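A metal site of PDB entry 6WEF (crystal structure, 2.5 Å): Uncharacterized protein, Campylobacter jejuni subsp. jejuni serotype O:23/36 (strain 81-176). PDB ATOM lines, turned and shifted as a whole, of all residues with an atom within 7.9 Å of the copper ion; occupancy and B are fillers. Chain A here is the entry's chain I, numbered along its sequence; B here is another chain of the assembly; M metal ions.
A ring nitrogen (NE2) of His 95 lies close to the side-chain carboxylate (OE2) of Glu 44 (3.3 Å).
ND1 of His 95 lies within hydrogen-bond range of O of Gly 93.
O of Leu 22 lies within hydrogen-bond range of N of His 42, at 2.8 Å.
A ring nitrogen (ND1) of His 42 is in hydrogen-bond range of the side-chain amide oxygen (OD1) of Asn 99 (2.9 Å).
The backbone NH of His 132 of chain B lies within hydrogen-bond range of the backbone carbonyl oxygen of Val 89 (3.1 Å).
A ring nitrogen (ND1) of His 132 of chain B sits at hydrogen-bond distance from the side-chain hydroxyl (OG1) of Thr 137 of chain B (2.8 Å).
N of Glu 44 is in hydrogen-bond range of O of Val 20.
Merely in contact with the copper ion: Glu 44 (3.2 Å).
Along chain A the residues within 4 Å of the copper ion span positions 42 to 95.
The nearest printed residue that does not touch the copper ion is Gly 97 (4.5 Å).
The copper ion is bound by a ring nitrogen (NE2) of His 95, a ring nitrogen (NE2) of His 42, a ring nitrogen (NE2) of His 132 of chain B and the side-chain sulfur of Met 88.
The copper ion has four donor atoms within binding distance.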
ATOM      1  N   VAL A  20       7.424   1.925 -31.847  1.00  0.00           N
ATOM      2  CA  VAL A  20       8.622   1.633 -32.630  1.00  0.00           C
ATOM      3  C   VAL A  20       9.150   0.269 -32.189  1.00  0.00           C
ATOM      4  O   VAL A  20       8.563  -0.397 -31.330  1.00  0.00           O
ATOM      5  CB  VAL A  20       9.699   2.727 -32.459  1.00  0.00           C
ATOM      6  CG1 VAL A  20       9.159   4.079 -32.885  1.00  0.00           C
ATOM      7  CG2 VAL A  20      10.201   2.779 -31.024  1.00  0.00           C
ATOM      8  N   LEU A  22      13.331  -1.615 -31.922  1.00  0.00           N
ATOM      9  CA  LEU A  22      14.744  -1.677 -32.232  1.00  0.00           C
ATOM     10  C   LEU A  22      15.209  -3.127 -32.119  1.00  0.00           C
ATOM     11  O   LEU A  22      14.410  -4.050 -31.955  1.00  0.00           O
ATOM     12  CB  LEU A  22      15.537  -0.776 -31.291  1.00  0.00           C
ATOM     13  CG  LEU A  22      15.257   0.724 -31.270  1.00  0.00           C
ATOM     14  CD1 LEU A  22      13.875   1.037 -30.710  1.00  0.00           C
ATOM     15  CD2 LEU A  22      16.324   1.428 -30.445  1.00  0.00           C
ATOM     16  N   ILE A  25      18.136  -4.713 -26.541  1.00  0.00           N
ATOM     17  CA  ILE A  25      18.829  -3.637 -25.821  1.00  0.00           C
ATOM     18  C   ILE A  25      19.244  -4.153 -24.447  1.00  0.00           C
ATOM     19  O   ILE A  25      18.494  -4.905 -23.808  1.00  0.00           O
ATOM     20  CB  ILE A  25      17.916  -2.395 -25.681  1.00  0.00           C
ATOM     21  CG1 ILE A  25      17.622  -1.788 -27.062  1.00  0.00           C
ATOM     22  CG2 ILE A  25      18.552  -1.387 -24.738  1.00  0.00           C
ATOM     23  CD1 ILE A  25      18.555  -0.669 -27.466  1.00  0.00           C
ATOM     24  N   GLU A  26      20.435  -3.766 -24.000  1.00  0.00           N
ATOM     25  CA  GLU A  26      20.870  -4.078 -22.642  1.00  0.00           C
ATOM     26  C   GLU A  26      20.269  -3.056 -21.682  1.00  0.00           C
ATOM     27  O   GLU A  26      20.403  -1.846 -21.878  1.00  0.00           O
ATOM     28  CB  GLU A  26      22.392  -4.080 -22.552  1.00  0.00           C
ATOM     29  CG  GLU A  26      23.026  -5.362 -23.074  1.00  0.00           C
ATOM     30  CD  GLU A  26      24.440  -5.164 -23.592  1.00  0.00           C
ATOM     31  OE1 GLU A  26      24.918  -6.021 -24.361  1.00  0.00           O
ATOM     32  OE2 GLU A  26      25.064  -4.138 -23.236  1.00  0.00           O
ATOM     33  N   MET A  27      19.623  -3.550 -20.625  1.00  0.00           N
ATOM     34  CA  MET A  27      18.833  -2.740 -19.725  1.00  0.00           C
ATOM     35  C   MET A  27      19.382  -2.852 -18.305  1.00  0.00           C
ATOM     36  O   MET A  27      19.772  -3.934 -17.870  1.00  0.00           O
ATOM     37  CB  MET A  27      17.365  -3.178 -19.769  1.00  0.00           C
ATOM     38  CG  MET A  27      16.345  -2.105 -19.412  1.00  0.00           C
ATOM     39  SD  MET A  27      14.948  -2.842 -18.529  1.00  0.00           S
ATOM     40  CE  MET A  27      13.809  -1.473 -18.410  1.00  0.00           C
ATOM     41  N   HIS A  42      13.346  -4.764 -29.518  1.00  0.00           N
ATOM     42  CA  HIS A  42      13.067  -3.948 -28.325  1.00  0.00           C
ATOM     43  C   HIS A  42      11.842  -3.087 -28.671  1.00  0.00           C
ATOM     44  O   HIS A  42      11.973  -2.006 -29.234  1.00  0.00           O
ATOM     45  CB  HIS A  42      14.258  -3.091 -27.941  1.00  0.00           C
ATOM     46  CG  HIS A  42      14.048  -2.299 -26.681  1.00  0.00           C
ATOM     47  ND1 HIS A  42      14.110  -2.863 -25.426  1.00  0.00           N
ATOM     48  CD2 HIS A  42      13.756  -0.994 -26.503  1.00  0.00           C
ATOM     49  CE1 HIS A  42      13.875  -1.929 -24.526  1.00  0.00           C
ATOM     50  NE2 HIS A  42      13.657  -0.783 -25.149  1.00  0.00           N
ATOM     51  N   LEU A  43      10.660  -3.598 -28.327  1.00  0.00           N
ATOM     52  CA  LEU A  43       9.427  -2.859 -28.569  1.00  0.00           C
ATOM     53  C   LEU A  43       9.322  -1.685 -27.617  1.00  0.00           C
ATOM     54  O   LEU A  43       9.516  -1.828 -26.409  1.00  0.00           O
ATOM     55  CB  LEU A  43       8.229  -3.791 -28.409  1.00  0.00           C
ATOM     56  CG  LEU A  43       6.847  -3.197 -28.685  1.00  0.00           C
ATOM     57  CD1 LEU A  43       6.793  -2.550 -30.060  1.00  0.00           C
ATOM     58  CD2 LEU A  43       5.779  -4.278 -28.551  1.00  0.00           C
ATOM     59  N   GLU A  44       9.032  -0.502 -28.163  1.00  0.00           N
ATOM     60  CA  GLU A  44       8.899   0.705 -27.368  1.00  0.00           C
ATOM     61  C   GLU A  44       7.564   1.379 -27.649  1.00  0.00           C
ATOM     62  O   GLU A  44       7.004   1.243 -28.736  1.00  0.00           O
ATOM     63  CB  GLU A  44      10.035   1.700 -27.656  1.00  0.00           C
ATOM     64  CG  GLU A  44      11.431   1.178 -27.369  1.00  0.00           C
ATOM     65  CD  GLU A  44      12.499   2.258 -27.503  1.00  0.00           C
ATOM     66  OE1 GLU A  44      12.127   3.433 -27.710  1.00  0.00           O
ATOM     67  OE2 GLU A  44      13.706   1.930 -27.418  1.00  0.00           O
ATOM     68  N   ALA A  45       7.069   2.101 -26.649  1.00  0.00           N
ATOM     69  CA  ALA A  45       5.828   2.874 -26.756  1.00  0.00           C
ATOM     70  C   ALA A  45       6.145   4.327 -26.422  1.00  0.00           C
ATOM     71  O   ALA A  45       6.482   4.640 -25.280  1.00  0.00           O
ATOM     72  CB  ALA A  45       4.754   2.307 -25.834  1.00  0.00           C
ATOM     73  N   ASP A  46       6.054   5.202 -27.415  1.00  0.00           N
ATOM     74  CA  ASP A  46       6.320   6.621 -27.246  1.00  0.00           C
ATOM     75  C   ASP A  46       5.002   7.344 -27.016  1.00  0.00           C
ATOM     76  O   ASP A  46       4.177   7.451 -27.927  1.00  0.00           O
ATOM     77  CB  ASP A  46       7.069   7.179 -28.458  1.00  0.00           C
ATOM     78  CG  ASP A  46       8.536   6.794 -28.481  1.00  0.00           C
ATOM     79  OD1 ASP A  46       9.159   6.765 -27.391  1.00  0.00           O
ATOM     80  OD2 ASP A  46       9.064   6.512 -29.573  1.00  0.00           O
ATOM     81  N   MET A  86       7.893  -1.573 -19.747  1.00  0.00           N
ATOM     82  CA  MET A  86       8.399  -0.987 -18.518  1.00  0.00           C
ATOM     83  C   MET A  86       9.028   0.374 -18.789  1.00  0.00           C
ATOM     84  O   MET A  86       9.648   0.581 -19.837  1.00  0.00           O
ATOM     85  CB  MET A  86       9.446  -1.909 -17.871  1.00  0.00           C
ATOM     86  CG  MET A  86       8.832  -3.069 -17.096  1.00  0.00           C
ATOM     87  SD  MET A  86       9.624  -4.647 -17.435  1.00  0.00           S
ATOM     88  CE  MET A  86       9.192  -4.879 -19.154  1.00  0.00           C
ATOM     89  N   PRO A  87       8.880   1.326 -17.863  1.00  0.00           N
ATOM     90  CA  PRO A  87       9.441   2.662 -18.099  1.00  0.00           C
ATOM     91  C   PRO A  87      10.955   2.658 -18.029  1.00  0.00           C
ATOM     92  O   PRO A  87      11.561   1.940 -17.227  1.00  0.00           O
ATOM     93  CB  PRO A  87       8.825   3.506 -16.977  1.00  0.00           C
ATOM     94  CG  PRO A  87       8.584   2.525 -15.868  1.00  0.00           C
ATOM     95  CD  PRO A  87       8.241   1.219 -16.538  1.00  0.00           C
ATOM     96  N   MET A  88      11.575   3.466 -18.883  1.00  0.00           N
ATOM     97  CA  MET A  88      13.026   3.528 -18.984  1.00  0.00           C
ATOM     98  C   MET A  88      13.400   4.789 -19.752  1.00  0.00           C
ATOM     99  O   MET A  88      12.535   5.523 -20.224  1.00  0.00           O
ATOM    100  CB  MET A  88      13.579   2.265 -19.660  1.00  0.00           C
ATOM    101  CG  MET A  88      12.951   1.984 -21.019  1.00  0.00           C
ATOM    102  SD  MET A  88      13.699   0.591 -21.860  1.00  0.00           S
ATOM    103  CE  MET A  88      12.621  -0.750 -21.344  1.00  0.00           C
ATOM    104  N   VAL A  89      14.705   5.027 -19.877  1.00  0.00           N
ATOM    105  CA  VAL A  89      15.220   6.190 -20.575  1.00  0.00           C
ATOM    106  C   VAL A  89      16.383   5.772 -21.456  1.00  0.00           C
ATOM    107  O   VAL A  89      17.187   4.917 -21.067  1.00  0.00           O
ATOM    108  CB  VAL A  89      15.652   7.304 -19.595  1.00  0.00           C
ATOM    109  CG1 VAL A  89      16.711   6.787 -18.624  1.00  0.00           C
ATOM    110  CG2 VAL A  89      16.169   8.519 -20.356  1.00  0.00           C
ATOM    111  N   ALA A  90      16.480   6.370 -22.633  1.00  0.00           N
ATOM    112  CA  ALA A  90      17.599   6.148 -23.538  1.00  0.00           C
ATOM    113  C   ALA A  90      18.214   7.499 -23.904  1.00  0.00           C
ATOM    114  O   ALA A  90      17.879   8.519 -23.303  1.00  0.00           O
ATOM    115  CB  ALA A  90      17.152   5.410 -24.796  1.00  0.00           C
ATOM    116  N   GLY A  93      15.375  10.036 -24.706  1.00  0.00           N
ATOM    117  CA  GLY A  93      14.346  10.400 -23.766  1.00  0.00           C
ATOM    118  C   GLY A  93      13.649   9.212 -23.124  1.00  0.00           C
ATOM    119  O   GLY A  93      13.799   8.065 -23.554  1.00  0.00           O
ATOM    120  N   PRO A  94      12.863   9.473 -22.081  1.00  0.00           N
ATOM    121  CA  PRO A  94      12.130   8.396 -21.423  1.00  0.00           C
ATOM    122  C   PRO A  94      11.076   7.779 -22.329  1.00  0.00           C
ATOM    123  O   PRO A  94      10.572   8.401 -23.273  1.00  0.00           O
ATOM    124  CB  PRO A  94      11.484   9.082 -20.213  1.00  0.00           C
ATOM    125  CG  PRO A  94      11.376  10.521 -20.613  1.00  0.00           C
ATOM    126  CD  PRO A  94      12.578  10.792 -21.471  1.00  0.00           C
ATOM    127  N   HIS A  95      10.723   6.540 -22.024  1.00  0.00           N
ATOM    128  CA  HIS A  95       9.754   5.794 -22.815  1.00  0.00           C
ATOM    129  C   HIS A  95       9.444   4.496 -22.078  1.00  0.00           C
ATOM    130  O   HIS A  95      10.017   4.194 -21.029  1.00  0.00           O
ATOM    131  CB  HIS A  95      10.289   5.516 -24.220  1.00  0.00           C
ATOM    132  CG  HIS A  95      11.477   4.605 -24.246  1.00  0.00           C
ATOM    133  ND1 HIS A  95      12.764   5.059 -24.078  1.00  0.00           N
ATOM    134  CD2 HIS A  95      11.574   3.268 -24.410  1.00  0.00           C
ATOM    135  CE1 HIS A  95      13.601   4.047 -24.145  1.00  0.00           C
ATOM    136  NE2 HIS A  95      12.904   2.943 -24.341  1.00  0.00           N
ATOM    137  N   TYR A  96       8.518   3.728 -22.647  1.00  0.00           N
ATOM    138  CA  TYR A  96       8.194   2.386 -22.190  1.00  0.00           C
ATOM    139  C   TYR A  96       8.661   1.381 -23.224  1.00  0.00           C
ATOM    140  O   TYR A  96       8.614   1.641 -24.432  1.00  0.00           O
ATOM    141  CB  TYR A  96       6.700   2.224 -21.949  1.00  0.00           C
ATOM    142  CG  TYR A  96       6.097   3.282 -21.041  1.00  0.00           C
ATOM    143  CD1 TYR A  96       6.037   3.093 -19.672  1.00  0.00           C
ATOM    144  CD2 TYR A  96       5.579   4.457 -21.566  1.00  0.00           C
ATOM    145  CE1 TYR A  96       5.493   4.056 -18.835  1.00  0.00           C
ATOM    146  CE2 TYR A  96       5.032   5.423 -20.743  1.00  0.00           C
ATOM    147  CZ  TYR A  96       4.984   5.221 -19.387  1.00  0.00           C
ATOM    148  OH  TYR A  96       4.445   6.183 -18.567  1.00  0.00           O
ATOM    149  N   GLY A  97       9.115   0.217 -22.762  1.00  0.00           N
ATOM    150  CA  GLY A  97       9.567  -0.796 -23.697  1.00  0.00           C
ATOM    151  C   GLY A  97       9.820  -2.122 -22.999  1.00  0.00           C
ATOM    152  O   GLY A  97       9.683  -2.238 -21.782  1.00  0.00           O
ATOM    153  N   ALA A  98      10.188  -3.111 -23.811  1.00  0.00           N
ATOM    154  CA  ALA A  98      10.486  -4.446 -23.305  1.00  0.00           C
ATOM    155  C   ALA A  98      11.280  -5.208 -24.353  1.00  0.00           C
ATOM    156  O   ALA A  98      11.177  -4.929 -25.549  1.00  0.00           O
ATOM    157  CB  ALA A  98       9.202  -5.208 -22.955  1.00  0.00           C
ATOM    158  N   ASN A  99      12.081  -6.155 -23.884  1.00  0.00           N
ATOM    159  CA  ASN A  99      12.824  -7.063 -24.754  1.00  0.00           C
ATOM    160  C   ASN A  99      11.983  -8.314 -25.002  1.00  0.00           C
ATOM    161  O   ASN A  99      11.551  -8.968 -24.047  1.00  0.00           O
ATOM    162  CB  ASN A  99      14.169  -7.442 -24.143  1.00  0.00           C
ATOM    163  CG  ASN A  99      15.276  -6.465 -24.524  1.00  0.00           C
ATOM    164  OD1 ASN A  99      15.098  -5.606 -25.378  1.00  0.00           O
ATOM    165  ND2 ASN A  99      16.417  -6.598 -23.862  1.00  0.00           N
ATOM    166  N   GLY B 130      14.034   1.760 -15.773  1.00  0.00           N
ATOM    167  CA  GLY B 130      15.122   1.197 -16.545  1.00  0.00           C
ATOM    168  C   GLY B 130      16.045   2.240 -17.140  1.00  0.00           C
ATOM    169  O   GLY B 130      15.822   3.448 -17.066  1.00  0.00           O
ATOM    170  N   ARG B 131      17.110   1.731 -17.754  1.00  0.00           N
ATOM    171  CA  ARG B 131      18.106   2.592 -18.397  1.00  0.00           C
ATOM    172  C   ARG B 131      18.815   1.787 -19.468  1.00  0.00           C
ATOM    173  O   ARG B 131      19.372   0.719 -19.169  1.00  0.00           O
ATOM    174  CB  ARG B 131      19.105   3.117 -17.360  1.00  0.00           C
ATOM    175  CG  ARG B 131      20.333   3.768 -17.986  1.00  0.00           C
ATOM    176  CD  ARG B 131      21.102   4.580 -16.967  1.00  0.00           C
ATOM    177  NE  ARG B 131      21.851   3.728 -16.042  1.00  0.00           N
ATOM    178  CZ  ARG B 131      23.107   3.331 -16.222  1.00  0.00           C
ATOM    179  NH1 ARG B 131      23.778   3.697 -17.303  1.00  0.00           N
ATOM    180  NH2 ARG B 131      23.691   2.553 -15.307  1.00  0.00           N
ATOM    181  N   HIS B 132      18.786   2.276 -20.694  1.00  0.00           N
ATOM    182  CA  HIS B 132      19.555   1.646 -21.761  1.00  0.00           C
ATOM    183  C   HIS B 132      21.047   1.819 -21.494  1.00  0.00           C
ATOM    184  O   HIS B 132      21.499   2.895 -21.099  1.00  0.00           O
ATOM    185  CB  HIS B 132      19.202   2.257 -23.118  1.00  0.00           C
ATOM    186  CG  HIS B 132      17.854   1.857 -23.631  1.00  0.00           C
ATOM    187  ND1 HIS B 132      17.523   1.879 -24.969  1.00  0.00           N
ATOM    188  CD2 HIS B 132      16.748   1.420 -22.972  1.00  0.00           C
ATOM    189  CE1 HIS B 132      16.279   1.482 -25.122  1.00  0.00           C
ATOM    190  NE2 HIS B 132      15.776   1.192 -23.927  1.00  0.00           N
ATOM    191  N   THR B 137      22.216   3.284 -28.033  1.00  0.00           N
ATOM    192  CA  THR B 137      21.159   4.062 -27.390  1.00  0.00           C
ATOM    193  C   THR B 137      21.360   4.242 -25.897  1.00  0.00           C
ATOM    194  O   THR B 137      20.534   4.891 -25.250  1.00  0.00           O
ATOM    195  CB  THR B 137      19.802   3.396 -27.642  1.00  0.00           C
ATOM    196  OG1 THR B 137      19.649   2.278 -26.761  1.00  0.00           O
ATOM    197  CG2 THR B 137      19.689   2.917 -29.083  1.00  0.00           C
HETATM  198 CU    CU M   1      13.643   1.092 -24.371  1.00  0.00          CU
